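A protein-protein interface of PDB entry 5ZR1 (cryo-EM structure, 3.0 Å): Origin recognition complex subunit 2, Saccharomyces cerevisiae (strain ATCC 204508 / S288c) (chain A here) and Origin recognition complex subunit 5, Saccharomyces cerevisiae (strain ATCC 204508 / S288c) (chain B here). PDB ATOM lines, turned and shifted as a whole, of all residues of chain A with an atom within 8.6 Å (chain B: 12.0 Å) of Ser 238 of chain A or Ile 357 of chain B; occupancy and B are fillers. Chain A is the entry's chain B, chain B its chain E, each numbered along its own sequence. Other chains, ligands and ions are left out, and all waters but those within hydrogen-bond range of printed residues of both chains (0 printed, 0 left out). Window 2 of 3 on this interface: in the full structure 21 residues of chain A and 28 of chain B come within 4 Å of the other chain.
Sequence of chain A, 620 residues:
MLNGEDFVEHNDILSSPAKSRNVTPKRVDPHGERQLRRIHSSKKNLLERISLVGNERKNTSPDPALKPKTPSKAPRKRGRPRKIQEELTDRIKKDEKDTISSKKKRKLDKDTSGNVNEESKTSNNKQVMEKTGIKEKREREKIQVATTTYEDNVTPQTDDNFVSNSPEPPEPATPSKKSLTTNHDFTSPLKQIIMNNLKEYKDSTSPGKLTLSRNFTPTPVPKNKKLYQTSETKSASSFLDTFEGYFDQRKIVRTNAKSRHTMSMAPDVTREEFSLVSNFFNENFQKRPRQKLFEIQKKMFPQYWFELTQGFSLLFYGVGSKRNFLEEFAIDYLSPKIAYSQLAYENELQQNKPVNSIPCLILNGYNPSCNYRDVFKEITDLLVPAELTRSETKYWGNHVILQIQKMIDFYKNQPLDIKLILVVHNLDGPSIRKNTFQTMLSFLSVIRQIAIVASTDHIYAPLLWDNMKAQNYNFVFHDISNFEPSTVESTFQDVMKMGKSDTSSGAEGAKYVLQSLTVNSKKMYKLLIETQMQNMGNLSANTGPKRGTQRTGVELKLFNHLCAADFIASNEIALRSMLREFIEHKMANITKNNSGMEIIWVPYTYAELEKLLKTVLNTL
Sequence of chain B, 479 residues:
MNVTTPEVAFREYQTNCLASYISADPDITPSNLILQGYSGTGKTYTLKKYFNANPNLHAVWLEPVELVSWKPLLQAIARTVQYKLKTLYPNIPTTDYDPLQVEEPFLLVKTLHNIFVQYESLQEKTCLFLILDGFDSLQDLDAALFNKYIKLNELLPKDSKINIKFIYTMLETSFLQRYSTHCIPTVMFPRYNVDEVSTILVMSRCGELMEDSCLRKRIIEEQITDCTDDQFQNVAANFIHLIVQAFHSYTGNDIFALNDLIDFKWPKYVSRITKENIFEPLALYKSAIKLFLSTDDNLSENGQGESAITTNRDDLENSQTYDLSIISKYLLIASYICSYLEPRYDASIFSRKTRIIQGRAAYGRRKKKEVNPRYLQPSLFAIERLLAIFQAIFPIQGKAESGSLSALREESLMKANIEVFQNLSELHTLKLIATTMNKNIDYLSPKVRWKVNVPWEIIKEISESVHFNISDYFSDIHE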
ATOM      1  N   ALA A 236       4.648   8.380  -5.304  1.00  0.00           N
ATOM      2  CA  ALA A 236       5.846   9.103  -5.713  1.00  0.00           C
ATOM      3  C   ALA A 236       6.600   8.338  -6.794  1.00  0.00           C
ATOM      4  O   ALA A 236       6.591   8.722  -7.963  1.00  0.00           O
ATOM      5  CB  ALA A 236       6.747   9.354  -4.515  1.00  0.00           C
ATOM      6  N   SER A 237       7.253   7.254  -6.393  1.00  0.00           N
ATOM      7  CA  SER A 237       8.019   6.428  -7.311  1.00  0.00           C
ATOM      8  C   SER A 237       7.173   5.264  -7.807  1.00  0.00           C
ATOM      9  O   SER A 237       6.226   4.833  -7.145  1.00  0.00           O
ATOM     10  CB  SER A 237       9.282   5.898  -6.634  1.00  0.00           C
ATOM     11  OG  SER A 237       8.958   5.002  -5.588  1.00  0.00           O
ATOM     12  N   SER A 238       7.528   4.755  -8.986  1.00  0.00           N
ATOM     13  CA  SER A 238       6.782   3.644  -9.563  1.00  0.00           C
ATOM     14  C   SER A 238       7.236   2.308  -8.991  1.00  0.00           C
ATOM     15  O   SER A 238       6.412   1.416  -8.766  1.00  0.00           O
ATOM     16  CB  SER A 238       6.920   3.653 -11.084  1.00  0.00           C
ATOM     17  OG  SER A 238       8.253   3.389 -11.472  1.00  0.00           O
ATOM     18  N   PHE A 239       8.533   2.155  -8.742  1.00  0.00           N
ATOM     19  CA  PHE A 239       9.074   0.940  -8.155  1.00  0.00           C
ATOM     20  C   PHE A 239       9.354   1.169  -6.678  1.00  0.00           C
ATOM     21  O   PHE A 239       9.736   2.266  -6.266  1.00  0.00           O
ATOM     22  CB  PHE A 239      10.360   0.509  -8.857  1.00  0.00           C
ATOM     23  CG  PHE A 239      10.212   0.318 -10.336  1.00  0.00           C
ATOM     24  CD1 PHE A 239       9.493  -0.748 -10.844  1.00  0.00           C
ATOM     25  CD2 PHE A 239      10.838   1.181 -11.219  1.00  0.00           C
ATOM     26  CE1 PHE A 239       9.367  -0.925 -12.205  1.00  0.00           C
ATOM     27  CE2 PHE A 239      10.724   1.002 -12.579  1.00  0.00           C
ATOM     28  CZ  PHE A 239       9.990  -0.052 -13.070  1.00  0.00           C
ATOM     29  N   LEU A 240       9.162   0.122  -5.880  1.00  0.00           N
ATOM     30  CA  LEU A 240       9.377   0.199  -4.440  1.00  0.00           C
ATOM     31  C   LEU A 240      10.514  -0.674  -3.946  1.00  0.00           C
ATOM     32  O   LEU A 240      11.319  -0.220  -3.132  1.00  0.00           O
ATOM     33  CB  LEU A 240       8.099  -0.169  -3.684  1.00  0.00           C
ATOM     34  CG  LEU A 240       6.983   0.865  -3.766  1.00  0.00           C
ATOM     35  CD1 LEU A 240       5.746   0.365  -3.058  1.00  0.00           C
ATOM     36  CD2 LEU A 240       7.452   2.166  -3.157  1.00  0.00           C
ATOM     37  N   ASP A 241      10.613  -1.919  -4.405  1.00  0.00           N
ATOM     38  CA  ASP A 241      11.722  -2.763  -3.992  1.00  0.00           C
ATOM     39  C   ASP A 241      12.256  -3.579  -5.159  1.00  0.00           C
ATOM     40  O   ASP A 241      11.512  -4.342  -5.777  1.00  0.00           O
ATOM     41  CB  ASP A 241      11.334  -3.682  -2.816  1.00  0.00           C
ATOM     42  CG  ASP A 241      10.152  -4.588  -3.100  1.00  0.00           C
ATOM     43  OD1 ASP A 241       9.378  -4.327  -4.031  1.00  0.00           O
ATOM     44  OD2 ASP A 241      10.035  -5.621  -2.417  1.00  0.00           O
ATOM     45  N   GLU A 244      15.694  -2.072  -9.093  1.00  0.00           N
ATOM     46  CA  GLU A 244      14.761  -1.158  -9.741  1.00  0.00           C
ATOM     47  C   GLU A 244      14.275  -0.089  -8.777  1.00  0.00           C
ATOM     48  O   GLU A 244      14.236   1.093  -9.122  1.00  0.00           O
ATOM     49  CB  GLU A 244      13.566  -1.936 -10.291  1.00  0.00           C
ATOM     50  CG  GLU A 244      13.891  -2.941 -11.375  1.00  0.00           C
ATOM     51  CD  GLU A 244      14.340  -2.292 -12.668  1.00  0.00           C
ATOM     52  OE1 GLU A 244      13.899  -1.163 -12.962  1.00  0.00           O
ATOM     53  OE2 GLU A 244      15.126  -2.924 -13.400  1.00  0.00           O
ATOM     54  N   GLY A 245      13.907  -0.487  -7.559  1.00  0.00           N
ATOM     55  CA  GLY A 245      13.469   0.486  -6.575  1.00  0.00           C
ATOM     56  C   GLY A 245      14.600   1.326  -6.025  1.00  0.00           C
ATOM     57  O   GLY A 245      14.375   2.450  -5.573  1.00  0.00           O
ATOM     58  N   ASP A 248      15.289   3.978  -8.897  1.00  0.00           N
ATOM     59  CA  ASP A 248      14.173   4.866  -9.187  1.00  0.00           C
ATOM     60  C   ASP A 248      13.840   5.801  -8.033  1.00  0.00           C
ATOM     61  O   ASP A 248      13.252   6.861  -8.265  1.00  0.00           O
ATOM     62  CB  ASP A 248      12.940   4.038  -9.562  1.00  0.00           C
ATOM     63  CG  ASP A 248      11.824   4.874 -10.135  1.00  0.00           C
ATOM     64  OD1 ASP A 248      11.943   5.317 -11.295  1.00  0.00           O
ATOM     65  OD2 ASP A 248      10.822   5.083  -9.425  1.00  0.00           O
ATOM     66  N   GLN A 249      14.204   5.453  -6.803  1.00  0.00           N
ATOM     67  CA  GLN A 249      13.922   6.327  -5.675  1.00  0.00           C
ATOM     68  C   GLN A 249      15.040   7.314  -5.380  1.00  0.00           C
ATOM     69  O   GLN A 249      14.843   8.217  -4.563  1.00  0.00           O
ATOM     70  CB  GLN A 249      13.628   5.509  -4.414  1.00  0.00           C
ATOM     71  CG  GLN A 249      12.290   4.798  -4.443  1.00  0.00           C
ATOM     72  CD  GLN A 249      11.974   4.104  -3.140  1.00  0.00           C
ATOM     73  OE1 GLN A 249      12.790   4.083  -2.222  1.00  0.00           O
ATOM     74  NE2 GLN A 249      10.778   3.543  -3.045  1.00  0.00           N
ATOM     75  N   LYS A 251      16.291   9.940  -6.946  1.00  0.00           N
ATOM     76  CA  LYS A 251      16.159  10.999  -7.931  1.00  0.00           C
ATOM     77  C   LYS A 251      16.555  12.340  -7.331  1.00  0.00           C
ATOM     78  O   LYS A 251      16.627  12.510  -6.111  1.00  0.00           O
ATOM     79  CB  LYS A 251      14.727  11.079  -8.464  1.00  0.00           C
ATOM     80  CG  LYS A 251      14.257   9.846  -9.197  1.00  0.00           C
ATOM     81  CD  LYS A 251      15.018   9.642 -10.491  1.00  0.00           C
ATOM     82  CE  LYS A 251      14.467   8.458 -11.262  1.00  0.00           C
ATOM     83  NZ  LYS A 251      15.232   8.201 -12.507  1.00  0.00           N
ATOM     84  N   ALA B 347      20.349   4.209 -13.506  1.00  0.00           N
ATOM     85  CA  ALA B 347      18.981   3.841 -13.842  1.00  0.00           C
ATOM     86  C   ALA B 347      18.758   3.749 -15.343  1.00  0.00           C
ATOM     87  O   ALA B 347      17.795   3.113 -15.774  1.00  0.00           O
ATOM     88  CB  ALA B 347      18.000   4.842 -13.238  1.00  0.00           C
ATOM     89  N   SER B 351      18.154  -0.698 -15.759  1.00  0.00           N
ATOM     90  CA  SER B 351      16.722  -0.907 -15.582  1.00  0.00           C
ATOM     91  C   SER B 351      16.115  -1.638 -16.772  1.00  0.00           C
ATOM     92  O   SER B 351      16.419  -1.343 -17.931  1.00  0.00           O
ATOM     93  CB  SER B 351      16.005   0.422 -15.368  1.00  0.00           C
ATOM     94  OG  SER B 351      16.413   1.023 -14.153  1.00  0.00           O
ATOM     95  N   ARG B 352      15.251  -2.604 -16.467  1.00  0.00           N
ATOM     96  CA  ARG B 352      14.653  -3.474 -17.467  1.00  0.00           C
ATOM     97  C   ARG B 352      13.168  -3.727 -17.264  1.00  0.00           C
ATOM     98  O   ARG B 352      12.523  -4.216 -18.196  1.00  0.00           O
ATOM     99  CB  ARG B 352      15.384  -4.822 -17.469  1.00  0.00           C
ATOM    100  CG  ARG B 352      15.148  -5.597 -16.185  1.00  0.00           C
ATOM    101  CD  ARG B 352      16.079  -6.774 -16.011  1.00  0.00           C
ATOM    102  NE  ARG B 352      17.448  -6.327 -15.790  1.00  0.00           N
ATOM    103  CZ  ARG B 352      18.477  -7.141 -15.586  1.00  0.00           C
ATOM    104  NH1 ARG B 352      18.290  -8.452 -15.545  1.00  0.00           N
ATOM    105  NH2 ARG B 352      19.690  -6.641 -15.399  1.00  0.00           N
ATOM    106  N   LYS B 353      12.597  -3.414 -16.105  1.00  0.00           N
ATOM    107  CA  LYS B 353      11.295  -3.943 -15.729  1.00  0.00           C
ATOM    108  C   LYS B 353      10.191  -2.960 -16.106  1.00  0.00           C
ATOM    109  O   LYS B 353      10.376  -1.742 -16.060  1.00  0.00           O
ATOM    110  CB  LYS B 353      11.268  -4.253 -14.227  1.00  0.00           C
ATOM    111  CG  LYS B 353      10.052  -5.034 -13.736  1.00  0.00           C
ATOM    112  CD  LYS B 353      10.205  -5.484 -12.286  1.00  0.00           C
ATOM    113  CE  LYS B 353      10.048  -4.322 -11.321  1.00  0.00           C
ATOM    114  NZ  LYS B 353      10.082  -4.734  -9.890  1.00  0.00           N
ATOM    115  N   THR B 354       9.043  -3.512 -16.503  1.00  0.00           N
ATOM    116  CA  THR B 354       7.921  -2.708 -16.964  1.00  0.00           C
ATOM    117  C   THR B 354       7.312  -1.903 -15.823  1.00  0.00           C
ATOM    118  O   THR B 354       7.375  -2.288 -14.654  1.00  0.00           O
ATOM    119  CB  THR B 354       6.844  -3.595 -17.588  1.00  0.00           C
ATOM    120  OG1 THR B 354       6.351  -4.510 -16.603  1.00  0.00           O
ATOM    121  CG2 THR B 354       7.411  -4.380 -18.756  1.00  0.00           C
ATOM    122  N   ARG B 355       6.710  -0.774 -16.182  1.00  0.00           N
ATOM    123  CA  ARG B 355       6.162   0.171 -15.219  1.00  0.00           C
ATOM    124  C   ARG B 355       4.647   0.025 -15.168  1.00  0.00           C
ATOM    125  O   ARG B 355       3.954   0.303 -16.151  1.00  0.00           O
ATOM    126  CB  ARG B 355       6.559   1.599 -15.585  1.00  0.00           C
ATOM    127  CG  ARG B 355       8.019   1.906 -15.345  1.00  0.00           C
ATOM    128  CD  ARG B 355       8.379   3.322 -15.739  1.00  0.00           C
ATOM    129  NE  ARG B 355       9.782   3.599 -15.455  1.00  0.00           N
ATOM    130  CZ  ARG B 355      10.218   4.120 -14.313  1.00  0.00           C
ATOM    131  NH1 ARG B 355       9.354   4.438 -13.362  1.00  0.00           N
ATOM    132  NH2 ARG B 355      11.511   4.335 -14.127  1.00  0.00           N
ATOM    133  N   ILE B 356       4.138  -0.418 -14.018  1.00  0.00           N
ATOM    134  CA  ILE B 356       2.707  -0.328 -13.756  1.00  0.00           C
ATOM    135  C   ILE B 356       2.303   1.127 -13.585  1.00  0.00           C
ATOM    136  O   ILE B 356       1.300   1.583 -14.146  1.00  0.00           O
ATOM    137  CB  ILE B 356       2.348  -1.155 -12.508  1.00  0.00           C
ATOM    138  CG1 ILE B 356       2.781  -2.605 -12.677  1.00  0.00           C
ATOM    139  CG2 ILE B 356       0.862  -1.107 -12.235  1.00  0.00           C
ATOM    140  CD1 ILE B 356       2.060  -3.338 -13.760  1.00  0.00           C
ATOM    141  N   ILE B 357       3.092   1.878 -12.829  1.00  0.00           N
ATOM    142  CA  ILE B 357       2.804   3.258 -12.464  1.00  0.00           C
ATOM    143  C   ILE B 357       3.619   4.181 -13.362  1.00  0.00           C
ATOM    144  O   ILE B 357       4.771   3.875 -13.697  1.00  0.00           O
ATOM    145  CB  ILE B 357       3.102   3.471 -10.964  1.00  0.00           C
ATOM    146  CG1 ILE B 357       2.127   2.644 -10.128  1.00  0.00           C
ATOM    147  CG2 ILE B 357       3.025   4.925 -10.542  1.00  0.00           C
ATOM    148  CD1 ILE B 357       2.461   2.610  -8.665  1.00  0.00           C
ATOM    149  N   GLN B 358       2.998   5.287 -13.784  1.00  0.00           N
ATOM    150  CA  GLN B 358       3.607   6.242 -14.703  1.00  0.00           C
ATOM    151  C   GLN B 358       4.884   6.856 -14.141  1.00  0.00           C
ATOM    152  O   GLN B 358       4.948   7.240 -12.970  1.00  0.00           O
ATOM    153  CB  GLN B 358       2.606   7.349 -15.027  1.00  0.00           C
ATOM    154  CG  GLN B 358       1.446   6.921 -15.905  1.00  0.00           C
ATOM    155  CD  GLN B 358       0.466   8.052 -16.156  1.00  0.00           C
ATOM    156  OE1 GLN B 358       0.592   9.136 -15.587  1.00  0.00           O
ATOM    157  NE2 GLN B 358      -0.511   7.806 -17.018  1.00  0.00           N
ATOM    158  N   GLY B 359       5.895   6.947 -14.991  1.00  0.00           N
ATOM    159  CA  GLY B 359       7.158   7.543 -14.613  1.00  0.00           C
ATOM    160  C   GLY B 359       8.098   7.501 -15.797  1.00  0.00           C
ATOM    161  O   GLY B 359       7.923   6.711 -16.730  1.00  0.00           O
ATOM    162  N   ARG B 360       9.097   8.374 -15.747  1.00  0.00           N
ATOM    163  CA  ARG B 360      10.073   8.492 -16.820  1.00  0.00           C
ATOM    164  C   ARG B 360      11.386   7.855 -16.390  1.00  0.00           C
ATOM    165  O   ARG B 360      11.849   8.073 -15.266  1.00  0.00           O
ATOM    166  CB  ARG B 360      10.292   9.955 -17.209  1.00  0.00           C
ATOM    167  CG  ARG B 360       9.058  10.630 -17.778  1.00  0.00           C
ATOM    168  CD  ARG B 360       9.350  12.061 -18.186  1.00  0.00           C
ATOM    169  NE  ARG B 360      10.245  12.116 -19.338  1.00  0.00           N
ATOM    170  CZ  ARG B 360       9.835  12.130 -20.600  1.00  0.00           C
ATOM    171  NH1 ARG B 360       8.539  12.108 -20.878  1.00  0.00           N
ATOM    172  NH2 ARG B 360      10.716  12.175 -21.588  1.00  0.00           N
ATOM    173  N   ALA B 361      11.975   7.067 -17.283  1.00  0.00           N
ATOM    174  CA  ALA B 361      13.273   6.475 -17.016  1.00  0.00           C
ATOM    175  C   ALA B 361      14.372   7.524 -17.152  1.00  0.00           C
ATOM    176  O   ALA B 361      14.167   8.611 -17.701  1.00  0.00           O
ATOM    177  CB  ALA B 361      13.535   5.308 -17.967  1.00  0.00           C
ATOM    178  N   ALA B 362      15.550   7.187 -16.634  1.00  0.00           N
ATOM    179  CA  ALA B 362      16.698   8.074 -16.746  1.00  0.00           C
ATOM    180  C   ALA B 362      17.175   8.133 -18.191  1.00  0.00           C
ATOM    181  O   ALA B 362      17.162   7.129 -18.908  1.00  0.00           O
ATOM    182  CB  ALA B 362      17.829   7.606 -15.833  1.00  0.00           C
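The side-chain hydroxyl (OG) of Ser 237 of chain A sits at hydrogen-bond distance from the backbone carbonyl oxygen (O) of Phe 239 of chain A, 2.9 Å away.
The backbone NH (N) of Ser 238 of chain A sits at hydrogen-bond distance from the side-chain carboxylate (OD2) of Asp 248 of chain A, at 3.3 Å.
The backbone carbonyl oxygen of Ala 347 of chain B sits at hydrogen-bond distance from the side-chain hydroxyl of Ser 351 of chain B (3.0 Å).
No residue of chain B comes within 4 Å of Ala 236 of chain A.
No residue of chain B comes within 4 Å of Ser 237 of chain A.
Of chain B, only Arg 355 (2.4 Å) and Ile 357 (3.4 Å) come within 4 Å of Ser 238 of chain A.
Of the printed residues of chain B, Phe 239 of chain A touches Lys 353 (3.5 Å), Thr 354 (3.4 Å) and Arg 355 (3.6 Å).
No residue of chain B comes within 4 Å of Leu 240 of chain A.
Asp 248 of chain A touches just one residue of chain B: Arg 355 (3.0 Å).
Printed residues of chain A within 4 Å of Arg 352 of chain B: Glu 244 (3.1 Å).
Printed residues of chain A within 4 Å of Thr 354 of chain B: Phe 239 (3.4 Å).
Printed residues of chain A within 4 Å of Ile 357 of chain B: Ser 238 (3.4 Å).
Gln 358 of chain B touches none of the printed residues of chain A.
Arg 360 of chain B touches none of the printed residues of chain A.
The nearest residue of chain B that does not touch Ser 238 of chain A is Gln 358 of chain B (4.5 Å).
The nearest printed residue of chain A that does not touch Thr 354 of chain B is Glu 244 of chain A (6.5 Å).
The side-chain hydroxyl (OG) of Ser 238 of chain A is in hydrogen-bond range of the guanidinium group (NH1) of Arg 355 of chain B (2.4 Å).
The side-chain carboxylate of Glu 244 of chain A sits at hydrogen-bond distance from the backbone NH of Arg 352 of chain B, 3.1 Å away.
The side-chain carboxylate (OD1) of Asp 248 of chain A is in salt-bridge range of the guanidinium group (NH2) of Arg 355 of chain B (3.0 Å).
Ser 238 of chain A touches Ile 357 of chain B (CB to O, 3.4 Å).
Lys 353 of chain B touches Phe 239 of chain A (O to CZ, 3.5 Å).
Thr 354 of chain B touches Phe 239 of chain A (O to CE1, 3.4 Å).
CG of Arg 355 of chain B touches CZ of Phe 239 of chain A, at 3.6 Å.
OE2 of Glu 244 of chain A touches CA of Ser 351 of chain B, at 3.4 Å.
Lys 353 of chain B touches Glu 244 of chain A (N to OE2, 3.7 Å).
Among the printed residues, Asp or Glu carboxylates within 4 Å of a Lys or Arg side-chain nitrogen of the other chain: Asp 248 of chain A with Arg 355 of chain B (3.0 Å).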
